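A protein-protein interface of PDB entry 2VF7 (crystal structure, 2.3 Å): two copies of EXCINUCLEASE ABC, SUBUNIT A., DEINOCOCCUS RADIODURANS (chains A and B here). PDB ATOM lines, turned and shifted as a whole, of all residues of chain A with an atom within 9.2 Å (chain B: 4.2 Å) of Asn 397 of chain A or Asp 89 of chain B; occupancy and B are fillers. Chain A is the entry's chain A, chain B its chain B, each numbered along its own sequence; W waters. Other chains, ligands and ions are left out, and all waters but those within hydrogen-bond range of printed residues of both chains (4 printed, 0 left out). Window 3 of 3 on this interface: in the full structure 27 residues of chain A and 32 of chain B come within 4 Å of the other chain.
The side-chain amide oxygen (OD1) of Asn 397 of chain A sits at hydrogen-bond distance from the guanidinium group (NH2) of Arg 64 of chain B, at 3.2 Å.
OD1 of Asn 397 of chain A sits close to O of Ile 88 of chain B (3.4 Å).
The side-chain hydroxyl of Ser 396 of chain A sits at hydrogen-bond distance from the backbone carbonyl oxygen of Gln 393 of chain A, 3.5 Å away.
OG of Ser 396 of chain A is in hydrogen-bond range of N of Leu 398 of chain A, at 3.1 Å.
The backbone carbonyl oxygen (O) of Leu 398 of chain A lies close to the side-chain amide oxygen (OD1) of Asn 432 of chain A (3.4 Å).
The backbone carbonyl oxygen (O) of Asp 89 of chain B sits at hydrogen-bond distance from the backbone NH (N) of Gln 17 of chain B, at 2.6 Å.
The guanidinium group (NH2) of Arg 19 of chain B is in salt-bridge range of the side-chain carboxylate (OD2) of Asp 89 of chain B, at 2.7 Å.
The backbone carbonyl oxygen (O) of Ile 88 of chain B lies within hydrogen-bond range of the guanidinium group (NH2) of Arg 64 of chain B (3.1 Å).
Among the printed residues, pairs that only touch across the chains: Phe 399 of chain A with Leu 91 of chain B (3.3 Å), Asn 397 of chain A with Asp 89 of chain B (3.6 Å), Ser 396 of chain A with Arg 64 of chain B (3.7 Å), Phe 399 of chain A with Gly 90 of chain B (3.9 Å) and Leu 398 of chain A with Arg 64 of chain B (3.9 Å).
Of chain B, only Arg 64, Ile 88 and Asp 89 come within 4 Å of Asn 397 of chain A.
Asp 89 of chain B touches just one residue of chain A: Asn 397 (3.6 Å).
No residue of chain A comes within 4 Å of Val 16 of chain B.
Printed residues of chain A within 4 Å of Gly 90 of chain B: Phe 399 (3.9 Å).
Of the printed residues of chain B, Leu 398 of chain A touches Arg 64.
Printed residues of chain B within 4 Å of Ser 396 of chain A: Arg 64.
Of the printed residues of chain A, Arg 64 of chain B touches Ser 396 (3.7 Å), Asn 397 (3.2 Å) and Leu 398 (3.9 Å).
Of the printed residues of chain B, Phe 399 of chain A touches Gly 90 (3.9 Å) and Leu 91 (3.3 Å).
Arg 359 of chain A touches none of the printed residues of chain B.
Gly 430 of chain A touches none of the printed residues of chain B.
The nearest printed residue of chain B that does not touch Asn 397 of chain A is Leu 91 of chain B (4.7 Å).
The nearest printed residue of chain A that does not touch Leu 91 of chain B is Asn 397 of chain A (4.7 Å).
Of the 9 printed residues of chain B, 5 touch a printed residue of chain A.
Of the 18 printed residues of chain A, 4 touch a printed residue of chain B.
Among the printed residues, 7 pairs touch across the chains.
Among the printed residues, no Asp or Glu carboxylate lies within 4 Å of a Lys or Arg side-chain nitrogen of the other chain.
No position is printed for both chains.
Water W4 lies within hydrogen-bond range of O of Phe 399 of chain A and O of Leu 91 of chain B.
Water W1 lies within hydrogen-bond range of the side-chain amide oxygen (OD1) of Asn 397 of chain A, the guanidinium group (NH2) of Arg 64 of chain B and the backbone NH (N) of Ile 88 of chain B.
Water W3 lies within hydrogen-bond range of O of Asn 397 of chain A (2.5 Å), NH1 of Arg 64 of chain B (2.7 Å), O of Ile 88 of chain B (2.9 Å) and N of Leu 91 of chain B (3.2 Å).
Water W2 lies within hydrogen-bond range of the backbone carbonyl oxygen (O) of Asn 397 of chain A (3.4 Å) and the backbone NH (N) of Gly 90 of chain B (3.4 Å).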
ATOM      1  N   LYS A 358      20.503   6.842   5.382  1.00  0.00           N
ATOM      2  CA  LYS A 358      19.327   6.947   6.245  1.00  0.00           C
ATOM      3  C   LYS A 358      19.745   7.552   7.582  1.00  0.00           C
ATOM      4  O   LYS A 358      19.107   8.482   8.080  1.00  0.00           O
ATOM      5  CB  LYS A 358      18.685   5.573   6.457  1.00  0.00           C
ATOM      6  CG  LYS A 358      17.384   5.576   7.278  1.00  0.00           C
ATOM      7  CD  LYS A 358      17.237   4.288   8.110  1.00  0.00           C
ATOM      8  CE  LYS A 358      18.302   4.205   9.227  1.00  0.00           C
ATOM      9  NZ  LYS A 358      18.350   2.872   9.901  1.00  0.00           N
ATOM     10  N   ARG A 359      20.820   7.013   8.148  1.00  0.00           N
ATOM     11  CA  ARG A 359      21.461   7.584   9.334  1.00  0.00           C
ATOM     12  C   ARG A 359      21.863   9.036   9.117  1.00  0.00           C
ATOM     13  O   ARG A 359      21.580   9.883   9.955  1.00  0.00           O
ATOM     14  CB  ARG A 359      22.683   6.765   9.740  1.00  0.00           C
ATOM     15  CG  ARG A 359      22.349   5.582  10.601  1.00  0.00           C
ATOM     16  CD  ARG A 359      23.350   4.463  10.428  1.00  0.00           C
ATOM     17  NE  ARG A 359      22.656   3.180  10.354  1.00  0.00           N
ATOM     18  CZ  ARG A 359      22.493   2.336  11.372  1.00  0.00           C
ATOM     19  NH1 ARG A 359      22.996   2.611  12.569  1.00  0.00           N
ATOM     20  NH2 ARG A 359      21.827   1.200  11.180  1.00  0.00           N
ATOM     21  N   ALA A 391      20.965  12.824  17.856  1.00  0.00           N
ATOM     22  CA  ALA A 391      20.830  12.218  16.543  1.00  0.00           C
ATOM     23  C   ALA A 391      21.141  10.731  16.607  1.00  0.00           C
ATOM     24  O   ALA A 391      20.416   9.917  16.026  1.00  0.00           O
ATOM     25  CB  ALA A 391      21.721  12.909  15.553  1.00  0.00           C
ATOM     26  N   THR A 392      22.190  10.375  17.351  1.00  0.00           N
ATOM     27  CA  THR A 392      22.648   8.975  17.454  1.00  0.00           C
ATOM     28  C   THR A 392      21.625   8.077  18.153  1.00  0.00           C
ATOM     29  O   THR A 392      21.505   6.884  17.844  1.00  0.00           O
ATOM     30  CB  THR A 392      24.012   8.895  18.176  1.00  0.00           C
ATOM     31  OG1 THR A 392      24.954   9.720  17.480  1.00  0.00           O
ATOM     32  CG2 THR A 392      24.532   7.483  18.200  1.00  0.00           C
ATOM     33  N   GLN A 393      20.898   8.669  19.094  1.00  0.00           N
ATOM     34  CA  GLN A 393      19.860   7.982  19.844  1.00  0.00           C
ATOM     35  C   GLN A 393      18.665   7.679  18.939  1.00  0.00           C
ATOM     36  O   GLN A 393      17.942   6.705  19.158  1.00  0.00           O
ATOM     37  CB  GLN A 393      19.376   8.847  21.016  1.00  0.00           C
ATOM     38  CG  GLN A 393      20.360   9.059  22.156  1.00  0.00           C
ATOM     39  CD  GLN A 393      21.325   7.896  22.408  1.00  0.00           C
ATOM     40  OE1 GLN A 393      20.963   6.848  22.966  1.00  0.00           O
ATOM     41  NE2 GLN A 393      22.577   8.099  22.014  1.00  0.00           N
ATOM     42  N   LEU A 394      18.460   8.539  17.941  1.00  0.00           N
ATOM     43  CA  LEU A 394      17.292   8.453  17.073  1.00  0.00           C
ATOM     44  C   LEU A 394      17.363   7.271  16.114  1.00  0.00           C
ATOM     45  O   LEU A 394      16.366   6.938  15.454  1.00  0.00           O
ATOM     46  CB  LEU A 394      17.051   9.769  16.329  1.00  0.00           C
ATOM     47  CG  LEU A 394      16.115  10.776  17.009  1.00  0.00           C
ATOM     48  CD1 LEU A 394      15.991  12.029  16.175  1.00  0.00           C
ATOM     49  CD2 LEU A 394      14.728  10.167  17.220  1.00  0.00           C
ATOM     50  N   TYR A 395      18.534   6.627  16.059  1.00  0.00           N
ATOM     51  CA  TYR A 395      18.704   5.381  15.322  1.00  0.00           C
ATOM     52  C   TYR A 395      19.387   4.285  16.130  1.00  0.00           C
ATOM     53  O   TYR A 395      20.017   3.391  15.571  1.00  0.00           O
ATOM     54  CB  TYR A 395      19.396   5.609  13.973  1.00  0.00           C
ATOM     55  CG  TYR A 395      20.749   6.307  13.975  1.00  0.00           C
ATOM     56  CD1 TYR A 395      21.922   5.617  14.303  1.00  0.00           C
ATOM     57  CD2 TYR A 395      20.863   7.642  13.569  1.00  0.00           C
ATOM     58  CE1 TYR A 395      23.166   6.249  14.265  1.00  0.00           C
ATOM     59  CE2 TYR A 395      22.103   8.282  13.527  1.00  0.00           C
ATOM     60  CZ  TYR A 395      23.246   7.579  13.873  1.00  0.00           C
ATOM     61  OH  TYR A 395      24.467   8.206  13.829  1.00  0.00           O
ATOM     62  N   SER A 396      19.234   4.342  17.447  1.00  0.00           N
ATOM     63  CA  SER A 396      19.970   3.446  18.321  1.00  0.00           C
ATOM     64  C   SER A 396      19.130   2.241  18.681  1.00  0.00           C
ATOM     65  O   SER A 396      19.676   1.207  19.076  1.00  0.00           O
ATOM     66  CB  SER A 396      20.397   4.166  19.595  1.00  0.00           C
ATOM     67  OG  SER A 396      19.469   3.928  20.638  1.00  0.00           O
ATOM     68  N   ASN A 397      17.808   2.400  18.559  1.00  0.00           N
ATOM     69  CA  ASN A 397      16.823   1.343  18.840  1.00  0.00           C
ATOM     70  C   ASN A 397      16.502   1.141  20.335  1.00  0.00           C
ATOM     71  O   ASN A 397      15.758   0.204  20.685  1.00  0.00           O
ATOM     72  CB  ASN A 397      17.226   0.008  18.180  1.00  0.00           C
ATOM     73  CG  ASN A 397      16.467  -0.280  16.885  1.00  0.00           C
ATOM     74  OD1 ASN A 397      16.400  -1.433  16.440  1.00  0.00           O
ATOM     75  ND2 ASN A 397      15.883   0.755  16.281  1.00  0.00           N
ATOM     76  N   LEU A 398      17.057   2.004  21.203  1.00  0.00           N
ATOM     77  CA  LEU A 398      16.717   2.006  22.642  1.00  0.00           C
ATOM     78  C   LEU A 398      15.244   2.314  22.892  1.00  0.00           C
ATOM     79  O   LEU A 398      14.684   3.224  22.265  1.00  0.00           O
ATOM     80  CB  LEU A 398      17.549   3.014  23.437  1.00  0.00           C
ATOM     81  CG  LEU A 398      18.742   2.538  24.252  1.00  0.00           C
ATOM     82  CD1 LEU A 398      18.907   3.411  25.501  1.00  0.00           C
ATOM     83  CD2 LEU A 398      18.582   1.085  24.649  1.00  0.00           C
ATOM     84  N   PHE A 399      14.656   1.572  23.837  1.00  0.00           N
ATOM     85  CA  PHE A 399      13.223   1.616  24.139  1.00  0.00           C
ATOM     86  C   PHE A 399      13.039   1.629  25.648  1.00  0.00           C
ATOM     87  O   PHE A 399      13.755   0.941  26.348  1.00  0.00           O
ATOM     88  CB  PHE A 399      12.504   0.392  23.543  1.00  0.00           C
ATOM     89  CG  PHE A 399      11.035   0.347  23.846  1.00  0.00           C
ATOM     90  CD1 PHE A 399      10.108   0.732  22.891  1.00  0.00           C
ATOM     91  CD2 PHE A 399      10.577  -0.064  25.097  1.00  0.00           C
ATOM     92  CE1 PHE A 399       8.738   0.711  23.165  1.00  0.00           C
ATOM     93  CE2 PHE A 399       9.217  -0.085  25.383  1.00  0.00           C
ATOM     94  CZ  PHE A 399       8.292   0.310  24.411  1.00  0.00           C
ATOM     95  N   GLY A 400      12.085   2.417  26.135  1.00  0.00           N
ATOM     96  CA  GLY A 400      11.758   2.482  27.552  1.00  0.00           C
ATOM     97  C   GLY A 400      12.808   3.064  28.491  1.00  0.00           C
ATOM     98  O   GLY A 400      12.947   2.582  29.599  1.00  0.00           O
ATOM     99  N   VAL A 401      13.565   4.073  28.062  1.00  0.00           N
ATOM    100  CA  VAL A 401      14.491   4.783  28.969  1.00  0.00           C
ATOM    101  C   VAL A 401      14.002   6.237  29.079  1.00  0.00           C
ATOM    102  O   VAL A 401      13.134   6.641  28.307  1.00  0.00           O
ATOM    103  CB  VAL A 401      16.009   4.743  28.498  1.00  0.00           C
ATOM    104  CG1 VAL A 401      16.589   3.357  28.556  1.00  0.00           C
ATOM    105  CG2 VAL A 401      16.201   5.342  27.110  1.00  0.00           C
ATOM    106  N   TYR A 403      15.514  10.077  28.701  1.00  0.00           N
ATOM    107  CA  TYR A 403      16.621  10.947  28.286  1.00  0.00           C
ATOM    108  C   TYR A 403      16.606  12.235  29.083  1.00  0.00           C
ATOM    109  O   TYR A 403      15.580  12.905  29.177  1.00  0.00           O
ATOM    110  CB  TYR A 403      16.541  11.247  26.795  1.00  0.00           C
ATOM    111  CG  TYR A 403      16.904  10.047  25.941  1.00  0.00           C
ATOM    112  CD1 TYR A 403      15.924   9.329  25.237  1.00  0.00           C
ATOM    113  CD2 TYR A 403      18.221   9.623  25.851  1.00  0.00           C
ATOM    114  CE1 TYR A 403      16.269   8.223  24.447  1.00  0.00           C
ATOM    115  CE2 TYR A 403      18.576   8.516  25.083  1.00  0.00           C
ATOM    116  CZ  TYR A 403      17.605   7.827  24.372  1.00  0.00           C
ATOM    117  OH  TYR A 403      17.999   6.744  23.604  1.00  0.00           O
ATOM    118  N   LEU A 427      11.996  11.010  19.156  1.00  0.00           N
ATOM    119  CA  LEU A 427      12.595  10.288  20.270  1.00  0.00           C
ATOM    120  C   LEU A 427      11.543   9.821  21.253  1.00  0.00           C
ATOM    121  O   LEU A 427      11.591   8.693  21.719  1.00  0.00           O
ATOM    122  CB  LEU A 427      13.618  11.166  21.007  1.00  0.00           C
ATOM    123  CG  LEU A 427      15.106  10.829  20.891  1.00  0.00           C
ATOM    124  CD1 LEU A 427      15.858  11.407  22.087  1.00  0.00           C
ATOM    125  CD2 LEU A 427      15.323   9.302  20.810  1.00  0.00           C
ATOM    126  N   GLY A 430       9.408   6.885  19.996  1.00  0.00           N
ATOM    127  CA  GLY A 430      10.100   5.592  19.976  1.00  0.00           C
ATOM    128  C   GLY A 430       9.901   4.742  21.229  1.00  0.00           C
ATOM    129  O   GLY A 430      10.426   3.631  21.316  1.00  0.00           O
ATOM    130  N   GLY A 431       9.150   5.281  22.193  1.00  0.00           N
ATOM    131  CA  GLY A 431       8.847   4.625  23.456  1.00  0.00           C
ATOM    132  C   GLY A 431       9.564   5.208  24.669  1.00  0.00           C
ATOM    133  O   GLY A 431       9.552   4.591  25.745  1.00  0.00           O
ATOM    134  N   ASN A 432      10.162   6.396  24.510  1.00  0.00           N
ATOM    135  CA  ASN A 432      10.996   7.023  25.552  1.00  0.00           C
ATOM    136  C   ASN A 432      10.352   8.246  26.230  1.00  0.00           C
ATOM    137  O   ASN A 432       9.336   8.757  25.771  1.00  0.00           O
ATOM    138  CB  ASN A 432      12.377   7.408  24.997  1.00  0.00           C
ATOM    139  CG  ASN A 432      13.009   6.310  24.152  1.00  0.00           C
ATOM    140  OD1 ASN A 432      13.359   5.241  24.644  1.00  0.00           O
ATOM    141  ND2 ASN A 432      13.163   6.583  22.861  1.00  0.00           N
ATOM    142  N   PHE B  15       5.070  -5.583  21.759  1.00  0.00           N
ATOM    143  CA  PHE B  15       5.918  -6.741  21.525  1.00  0.00           C
ATOM    144  C   PHE B  15       7.366  -6.354  21.278  1.00  0.00           C
ATOM    145  O   PHE B  15       7.649  -5.309  20.694  1.00  0.00           O
ATOM    146  CB  PHE B  15       5.407  -7.533  20.307  1.00  0.00           C
ATOM    147  CG  PHE B  15       4.154  -8.311  20.567  1.00  0.00           C
ATOM    148  CD1 PHE B  15       2.911  -7.768  20.280  1.00  0.00           C
ATOM    149  CD2 PHE B  15       4.213  -9.601  21.085  1.00  0.00           C
ATOM    150  CE1 PHE B  15       1.742  -8.497  20.517  1.00  0.00           C
ATOM    151  CE2 PHE B  15       3.054 -10.329  21.329  1.00  0.00           C
ATOM    152  CZ  PHE B  15       1.816  -9.775  21.044  1.00  0.00           C
ATOM    153  N   VAL B  16       8.267  -7.223  21.731  1.00  0.00           N
ATOM    154  CA  VAL B  16       9.669  -7.189  21.343  1.00  0.00           C
ATOM    155  C   VAL B  16       9.756  -7.956  20.024  1.00  0.00           C
ATOM    156  O   VAL B  16       9.221  -9.058  19.913  1.00  0.00           O
ATOM    157  CB  VAL B  16      10.562  -7.832  22.432  1.00  0.00           C
ATOM    158  CG1 VAL B  16      12.035  -7.818  22.033  1.00  0.00           C
ATOM    159  CG2 VAL B  16      10.356  -7.131  23.763  1.00  0.00           C
ATOM    160  N   GLN B  17      10.404  -7.360  19.027  1.00  0.00           N
ATOM    161  CA  GLN B  17      10.432  -7.903  17.665  1.00  0.00           C
ATOM    162  C   GLN B  17      11.857  -8.216  17.246  1.00  0.00           C
ATOM    163  O   GLN B  17      12.633  -7.311  16.937  1.00  0.00           O
ATOM    164  CB  GLN B  17       9.820  -6.904  16.682  1.00  0.00           C
ATOM    165  CG  GLN B  17       9.492  -7.466  15.310  1.00  0.00           C
ATOM    166  CD  GLN B  17       8.166  -8.227  15.284  1.00  0.00           C
ATOM    167  OE1 GLN B  17       7.158  -7.760  15.831  1.00  0.00           O
ATOM    168  NE2 GLN B  17       8.162  -9.401  14.650  1.00  0.00           N
ATOM    169  N   ARG B  19      14.460 -10.020  14.606  1.00  0.00           N
ATOM    170  CA  ARG B  19      14.576 -10.351  13.204  1.00  0.00           C
ATOM    171  C   ARG B  19      16.040 -10.622  12.909  1.00  0.00           C
ATOM    172  O   ARG B  19      16.917  -9.904  13.395  1.00  0.00           O
ATOM    173  CB  ARG B  19      14.020  -9.213  12.329  1.00  0.00           C
ATOM    174  CG  ARG B  19      12.493  -9.288  12.104  1.00  0.00           C
ATOM    175  CD  ARG B  19      11.869  -8.001  11.542  1.00  0.00           C
ATOM    176  NE  ARG B  19      12.007  -6.879  12.472  1.00  0.00           N
ATOM    177  CZ  ARG B  19      12.691  -5.770  12.208  1.00  0.00           C
ATOM    178  NH1 ARG B  19      13.287  -5.619  11.024  1.00  0.00           N
ATOM    179  NH2 ARG B  19      12.774  -4.805  13.121  1.00  0.00           N
ATOM    180  N   ARG B  64      23.452  -1.986  23.982  1.00  0.00           N
ATOM    181  CA  ARG B  64      22.819  -0.740  23.537  1.00  0.00           C
ATOM    182  C   ARG B  64      22.706   0.325  24.616  1.00  0.00           C
ATOM    183  O   ARG B  64      22.597   1.512  24.316  1.00  0.00           O
ATOM    184  CB  ARG B  64      21.414  -1.015  23.040  1.00  0.00           C
ATOM    185  CG  ARG B  64      21.314  -1.737  21.743  1.00  0.00           C
ATOM    186  CD  ARG B  64      19.873  -2.044  21.558  1.00  0.00           C
ATOM    187  NE  ARG B  64      19.536  -2.372  20.186  1.00  0.00           N
ATOM    188  CZ  ARG B  64      18.368  -2.892  19.827  1.00  0.00           C
ATOM    189  NH1 ARG B  64      17.437  -3.142  20.746  1.00  0.00           N
ATOM    190  NH2 ARG B  64      18.129  -3.168  18.552  1.00  0.00           N
ATOM    191  N   ILE B  88      16.192  -5.745  16.660  1.00  0.00           N
ATOM    192  CA  ILE B  88      15.306  -5.942  17.816  1.00  0.00           C
ATOM    193  C   ILE B  88      14.521  -4.661  18.130  1.00  0.00           C
ATOM    194  O   ILE B  88      15.076  -3.703  18.658  1.00  0.00           O
ATOM    195  CB  ILE B  88      16.061  -6.407  19.089  1.00  0.00           C
ATOM    196  CG1 ILE B  88      17.022  -7.548  18.762  1.00  0.00           C
ATOM    197  CG2 ILE B  88      15.060  -6.821  20.170  1.00  0.00           C
ATOM    198  CD1 ILE B  88      18.042  -7.833  19.803  1.00  0.00           C
ATOM    199  N   ASP B  89      13.236  -4.643  17.798  1.00  0.00           N
ATOM    200  CA  ASP B  89      12.376  -3.549  18.225  1.00  0.00           C
ATOM    201  C   ASP B  89      11.693  -3.891  19.540  1.00  0.00           C
ATOM    202  O   ASP B  89      11.422  -5.057  19.819  1.00  0.00           O
ATOM    203  CB  ASP B  89      11.329  -3.240  17.157  1.00  0.00           C
ATOM    204  CG  ASP B  89      11.942  -3.050  15.784  1.00  0.00           C
ATOM    205  OD1 ASP B  89      13.149  -2.703  15.723  1.00  0.00           O
ATOM    206  OD2 ASP B  89      11.223  -3.247  14.769  1.00  0.00           O
ATOM    207  N   GLY B  90      11.435  -2.872  20.347  1.00  0.00           N
ATOM    208  CA  GLY B  90      10.591  -3.004  21.520  1.00  0.00           C
ATOM    209  C   GLY B  90      11.291  -3.418  22.794  1.00  0.00           C
ATOM    210  O   GLY B  90      10.629  -3.699  23.789  1.00  0.00           O
ATOM    211  N   LEU B  91      12.622  -3.438  22.763  1.00  0.00           N
ATOM    212  CA  LEU B  91      13.440  -4.043  23.826  1.00  0.00           C
ATOM    213  C   LEU B  91      13.833  -3.036  24.910  1.00  0.00           C
ATOM    214  O   LEU B  91      14.476  -2.025  24.597  1.00  0.00           O
ATOM    215  CB  LEU B  91      14.717  -4.645  23.221  1.00  0.00           C
ATOM    216  CG  LEU B  91      15.415  -5.927  23.714  1.00  0.00           C
ATOM    217  CD1 LEU B  91      16.905  -5.772  23.439  1.00  0.00           C
ATOM    218  CD2 LEU B  91      15.194  -6.279  25.183  1.00  0.00           C
HETATM  219  O   HOH W   1      17.773  -3.445  16.006  1.00  0.00           O
HETATM  220  O   HOH W   2      12.767   0.048  19.145  1.00  0.00           O
HETATM  221  O   HOH W   3      14.966  -2.125  21.050  1.00  0.00           O
HETATM  222  O   HOH W   4      15.928   0.142  25.570  1.00  0.00           O
